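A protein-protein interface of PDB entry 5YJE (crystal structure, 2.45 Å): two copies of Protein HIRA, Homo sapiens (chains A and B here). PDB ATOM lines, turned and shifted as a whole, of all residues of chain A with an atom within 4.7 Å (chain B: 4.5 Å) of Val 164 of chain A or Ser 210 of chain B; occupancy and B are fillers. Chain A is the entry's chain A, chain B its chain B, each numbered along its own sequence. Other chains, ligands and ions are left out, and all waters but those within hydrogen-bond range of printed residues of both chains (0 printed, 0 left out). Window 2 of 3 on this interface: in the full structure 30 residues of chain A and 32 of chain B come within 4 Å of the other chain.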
ATOM      1  N   VAL A 156       4.710 -32.552 -15.786  1.00  0.00           N
ATOM      2  CA  VAL A 156       5.752 -31.582 -16.107  1.00  0.00           C
ATOM      3  C   VAL A 156       5.158 -30.187 -16.006  1.00  0.00           C
ATOM      4  O   VAL A 156       4.147 -29.886 -16.652  1.00  0.00           O
ATOM      5  CB  VAL A 156       6.347 -31.776 -17.516  1.00  0.00           C
ATOM      6  CG1 VAL A 156       7.459 -30.756 -17.741  1.00  0.00           C
ATOM      7  CG2 VAL A 156       6.848 -33.189 -17.720  1.00  0.00           C
ATOM      8  N   TRP A 157       5.806 -29.326 -15.228  1.00  0.00           N
ATOM      9  CA  TRP A 157       5.425 -27.930 -15.114  1.00  0.00           C
ATOM     10  C   TRP A 157       6.535 -27.038 -15.658  1.00  0.00           C
ATOM     11  O   TRP A 157       7.723 -27.359 -15.573  1.00  0.00           O
ATOM     12  CB  TRP A 157       5.117 -27.561 -13.651  1.00  0.00           C
ATOM     13  CG  TRP A 157       3.963 -28.329 -13.095  1.00  0.00           C
ATOM     14  CD1 TRP A 157       2.650 -28.039 -13.264  1.00  0.00           C
ATOM     15  CD2 TRP A 157       4.011 -29.518 -12.298  1.00  0.00           C
ATOM     16  NE1 TRP A 157       1.874 -28.968 -12.632  1.00  0.00           N
ATOM     17  CE2 TRP A 157       2.680 -29.892 -12.030  1.00  0.00           C
ATOM     18  CE3 TRP A 157       5.046 -30.304 -11.787  1.00  0.00           C
ATOM     19  CZ2 TRP A 157       2.350 -31.011 -11.261  1.00  0.00           C
ATOM     20  CZ3 TRP A 157       4.718 -31.417 -11.014  1.00  0.00           C
ATOM     21  CH2 TRP A 157       3.386 -31.756 -10.757  1.00  0.00           C
ATOM     22  N   GLN A 162       4.711 -20.691 -15.199  1.00  0.00           N
ATOM     23  CA  GLN A 162       3.637 -21.053 -14.259  1.00  0.00           C
ATOM     24  C   GLN A 162       2.481 -21.749 -14.969  1.00  0.00           C
ATOM     25  O   GLN A 162       1.308 -21.481 -14.698  1.00  0.00           O
ATOM     26  CB  GLN A 162       3.140 -19.842 -13.468  1.00  0.00           C
ATOM     27  CG  GLN A 162       4.280 -19.143 -12.751  1.00  0.00           C
ATOM     28  CD  GLN A 162       3.793 -18.042 -11.858  1.00  0.00           C
ATOM     29  OE1 GLN A 162       4.382 -17.779 -10.810  1.00  0.00           O
ATOM     30  NE2 GLN A 162       2.698 -17.394 -12.257  1.00  0.00           N
ATOM     31  N   VAL A 163       2.821 -22.649 -15.887  1.00  0.00           N
ATOM     32  CA  VAL A 163       1.846 -23.434 -16.628  1.00  0.00           C
ATOM     33  C   VAL A 163       2.253 -24.891 -16.527  1.00  0.00           C
ATOM     34  O   VAL A 163       3.436 -25.221 -16.406  1.00  0.00           O
ATOM     35  CB  VAL A 163       1.728 -23.019 -18.122  1.00  0.00           C
ATOM     36  CG1 VAL A 163       1.096 -21.648 -18.264  1.00  0.00           C
ATOM     37  CG2 VAL A 163       3.102 -23.056 -18.799  1.00  0.00           C
ATOM     38  N   VAL A 164       1.255 -25.762 -16.583  1.00  0.00           N
ATOM     39  CA  VAL A 164       1.517 -27.176 -16.774  1.00  0.00           C
ATOM     40  C   VAL A 164       1.957 -27.409 -18.218  1.00  0.00           C
ATOM     41  O   VAL A 164       1.497 -26.729 -19.151  1.00  0.00           O
ATOM     42  CB  VAL A 164       0.260 -27.988 -16.421  1.00  0.00           C
ATOM     43  CG1 VAL A 164      -0.846 -27.671 -17.397  1.00  0.00           C
ATOM     44  CG2 VAL A 164       0.560 -29.479 -16.337  1.00  0.00           C
ATOM     45  N   VAL A 165       2.890 -28.336 -18.403  1.00  0.00           N
ATOM     46  CA  VAL A 165       3.312 -28.777 -19.716  1.00  0.00           C
ATOM     47  C   VAL A 165       2.779 -30.170 -20.017  1.00  0.00           C
ATOM     48  O   VAL A 165       2.237 -30.421 -21.092  1.00  0.00           O
ATOM     49  CB  VAL A 165       4.849 -28.734 -19.840  1.00  0.00           C
ATOM     50  CG1 VAL A 165       5.285 -29.345 -21.178  1.00  0.00           C
ATOM     51  CG2 VAL A 165       5.330 -27.314 -19.690  1.00  0.00           C
ATOM     52  N   VAL A 166       2.912 -31.085 -19.065  1.00  0.00           N
ATOM     53  CA  VAL A 166       2.396 -32.436 -19.202  1.00  0.00           C
ATOM     54  C   VAL A 166       1.544 -32.699 -17.976  1.00  0.00           C
ATOM     55  O   VAL A 166       2.067 -32.754 -16.859  1.00  0.00           O
ATOM     56  CB  VAL A 166       3.511 -33.476 -19.326  1.00  0.00           C
ATOM     57  CG1 VAL A 166       2.908 -34.874 -19.410  1.00  0.00           C
ATOM     58  CG2 VAL A 166       4.392 -33.173 -20.544  1.00  0.00           C
ATOM     59  N   LYS A 167       0.231 -32.853 -18.177  1.00  0.00           N
ATOM     60  CA  LYS A 167      -0.730 -33.042 -17.092  1.00  0.00           C
ATOM     61  C   LYS A 167      -0.997 -34.525 -16.850  1.00  0.00           C
ATOM     62  O   LYS A 167      -1.877 -35.118 -17.482  1.00  0.00           O
ATOM     63  CB  LYS A 167      -2.044 -32.320 -17.382  1.00  0.00           C
ATOM     64  CG  LYS A 167      -3.010 -32.516 -16.229  1.00  0.00           C
ATOM     65  CD  LYS A 167      -4.243 -31.688 -16.369  1.00  0.00           C
ATOM     66  CE  LYS A 167      -5.215 -31.928 -15.200  1.00  0.00           C
ATOM     67  NZ  LYS A 167      -4.643 -31.540 -13.869  1.00  0.00           N
ATOM     68  N   GLU B 169     -11.780 -32.297 -12.265  1.00  0.00           N
ATOM     69  CA  GLU B 169     -10.701 -32.663 -11.346  1.00  0.00           C
ATOM     70  C   GLU B 169     -11.256 -33.500 -10.216  1.00  0.00           C
ATOM     71  O   GLU B 169     -12.184 -33.074  -9.525  1.00  0.00           O
ATOM     72  CB  GLU B 169     -10.018 -31.427 -10.780  1.00  0.00           C
ATOM     73  CG  GLU B 169      -9.231 -30.716 -11.825  1.00  0.00           C
ATOM     74  CD  GLU B 169      -8.070 -31.558 -12.359  1.00  0.00           C
ATOM     75  OE1 GLU B 169      -7.373 -32.223 -11.555  1.00  0.00           O
ATOM     76  OE2 GLU B 169      -7.851 -31.532 -13.584  1.00  0.00           O
ATOM     77  N   PHE B 205      -7.585 -24.880  -6.574  1.00  0.00           N
ATOM     78  CA  PHE B 205      -7.151 -25.436  -7.849  1.00  0.00           C
ATOM     79  C   PHE B 205      -6.672 -24.299  -8.745  1.00  0.00           C
ATOM     80  O   PHE B 205      -7.423 -23.362  -9.026  1.00  0.00           O
ATOM     81  CB  PHE B 205      -8.249 -26.240  -8.547  1.00  0.00           C
ATOM     82  CG  PHE B 205      -7.724 -27.050  -9.695  1.00  0.00           C
ATOM     83  CD1 PHE B 205      -7.234 -28.324  -9.492  1.00  0.00           C
ATOM     84  CD2 PHE B 205      -7.645 -26.502 -10.964  1.00  0.00           C
ATOM     85  CE1 PHE B 205      -6.689 -29.060 -10.557  1.00  0.00           C
ATOM     86  CE2 PHE B 205      -7.124 -27.226 -12.012  1.00  0.00           C
ATOM     87  CZ  PHE B 205      -6.638 -28.510 -11.807  1.00  0.00           C
ATOM     88  N   ASN B 206      -5.422 -24.379  -9.187  1.00  0.00           N
ATOM     89  CA  ASN B 206      -4.908 -23.368 -10.084  1.00  0.00           C
ATOM     90  C   ASN B 206      -5.134 -23.831 -11.513  1.00  0.00           C
ATOM     91  O   ASN B 206      -4.692 -24.930 -11.868  1.00  0.00           O
ATOM     92  CB  ASN B 206      -3.429 -23.104  -9.836  1.00  0.00           C
ATOM     93  CG  ASN B 206      -2.925 -21.887 -10.608  1.00  0.00           C
ATOM     94  OD1 ASN B 206      -2.174 -22.019 -11.571  1.00  0.00           O
ATOM     95  ND2 ASN B 206      -3.393 -20.697 -10.218  1.00  0.00           N
ATOM     96  N   PRO B 207      -5.841 -23.063 -12.343  1.00  0.00           N
ATOM     97  CA  PRO B 207      -6.150 -23.569 -13.696  1.00  0.00           C
ATOM     98  C   PRO B 207      -4.945 -23.592 -14.617  1.00  0.00           C
ATOM     99  O   PRO B 207      -4.811 -24.519 -15.422  1.00  0.00           O
ATOM    100  CB  PRO B 207      -7.252 -22.615 -14.189  1.00  0.00           C
ATOM    101  CG  PRO B 207      -7.829 -22.002 -12.948  1.00  0.00           C
ATOM    102  CD  PRO B 207      -6.623 -21.862 -12.011  1.00  0.00           C
ATOM    103  N   SER B 208      -4.022 -22.643 -14.477  1.00  0.00           N
ATOM    104  CA  SER B 208      -2.833 -22.640 -15.324  1.00  0.00           C
ATOM    105  C   SER B 208      -1.856 -23.746 -14.936  1.00  0.00           C
ATOM    106  O   SER B 208      -1.322 -24.452 -15.804  1.00  0.00           O
ATOM    107  CB  SER B 208      -2.157 -21.276 -15.237  1.00  0.00           C
ATOM    108  OG  SER B 208      -3.018 -20.277 -15.740  1.00  0.00           O
ATOM    109  N   LEU B 209      -1.550 -23.880 -13.639  1.00  0.00           N
ATOM    110  CA  LEU B 209      -0.667 -24.977 -13.257  1.00  0.00           C
ATOM    111  C   LEU B 209      -1.391 -26.311 -13.364  1.00  0.00           C
ATOM    112  O   LEU B 209      -0.746 -27.349 -13.564  1.00  0.00           O
ATOM    113  CB  LEU B 209      -0.127 -24.785 -11.842  1.00  0.00           C
ATOM    114  CG  LEU B 209       1.083 -23.896 -11.534  1.00  0.00           C
ATOM    115  CD1 LEU B 209       1.387 -23.999 -10.051  1.00  0.00           C
ATOM    116  CD2 LEU B 209       2.344 -24.222 -12.375  1.00  0.00           C
ATOM    117  N   SER B 210      -2.727 -26.293 -13.242  1.00  0.00           N
ATOM    118  CA  SER B 210      -3.558 -27.497 -13.283  1.00  0.00           C
ATOM    119  C   SER B 210      -3.300 -28.378 -12.067  1.00  0.00           C
ATOM    120  O   SER B 210      -3.193 -29.600 -12.168  1.00  0.00           O
ATOM    121  CB  SER B 210      -3.371 -28.279 -14.585  1.00  0.00           C
ATOM    122  OG  SER B 210      -4.595 -28.887 -14.952  1.00  0.00           O
ATOM    123  N   THR B 211      -3.245 -27.745 -10.900  1.00  0.00           N
ATOM    124  CA  THR B 211      -2.827 -28.383  -9.663  1.00  0.00           C
ATOM    125  C   THR B 211      -3.771 -28.006  -8.532  1.00  0.00           C
ATOM    126  O   THR B 211      -4.287 -26.886  -8.466  1.00  0.00           O
ATOM    127  CB  THR B 211      -1.388 -27.963  -9.246  1.00  0.00           C
ATOM    128  OG1 THR B 211      -1.283 -26.535  -9.283  1.00  0.00           O
ATOM    129  CG2 THR B 211      -0.322 -28.567 -10.148  1.00  0.00           C
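Hydrophobic or aromatic side chains of chain B that line the printed part of chain A: Leu 209.
Printed residues of chain A that touch a printed residue of chain B: Trp 157, Gln 162, Val 163, Val 164 and Lys 167.
Hydrophobic or aromatic side chains of chain A that line the printed part of chain B: Trp 157 and Val 164.
Among the printed residues, 11 pairs touch across the chains.
Val 156 of chain A touches none of the printed residues of chain B.
Of the printed residues of chain B, Trp 157 of chain A touches Leu 209 (3.2 Å) and Thr 211 (3.3 Å).
Of chain B, only Ser 208, Leu 209 and Ser 210 come within 4 Å of Val 164 of chain A.
Val 166 of chain A touches none of the printed residues of chain B.
Ser 210 of chain B touches just these residues of chain A: Val 164 (3.8 Å) and Lys 167 (2.9 Å).
Of the printed residues of chain A, Thr 211 of chain B touches Trp 157.
The side-chain hydroxyl (OG) of Ser 210 of chain B is in hydrogen-bond range of the side-chain amino group (NZ) of Lys 167 of chain A (2.9 Å).
The backbone NH (N) of Val 164 of chain A lies within hydrogen-bond range of the backbone carbonyl oxygen (O) of Ser 208 of chain B (3.0 Å).
The side-chain amino group of Lys 167 of chain A is in salt-bridge range of the side-chain carboxylate of Glu 169 of chain B, 3.2 Å away.
NE1 of Trp 157 of chain A lies within hydrogen-bond range of O of Leu 209 of chain B (3.2 Å).
Trp 157 of chain A touches Thr 211 of chain B.
Ser 208 of chain B touches Gln 162 of chain A.
Leu 209 of chain B touches Gln 162 of chain A (CD2 to C, 3.6 Å).
Ser 208 of chain B touches Val 163 of chain A.
Val 163 of chain A touches Leu 209 of chain B.
Val 164 of chain A touches Leu 209 of chain B (CB to O, 3.1 Å).
Val 164 of chain A touches Ser 210 of chain B (CG1 to CB, 3.8 Å).
No position is printed for both chains.
Of the 11 pairs that touch across the chains among the printed residues, none has its exchanged pair printed and touching as well.
OD1 of Asn 206 of chain B is in hydrogen-bond range of N of Leu 209 of chain B (2.9 Å).
The backbone carbonyl oxygen (O) of Thr 211 of chain B lies within hydrogen-bond range of the backbone NH (N) of Asn 206 of chain B, at 2.8 Å.
OD1 of Asn 206 of chain B sits close to N of Ser 208 of chain B (3.5 Å).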
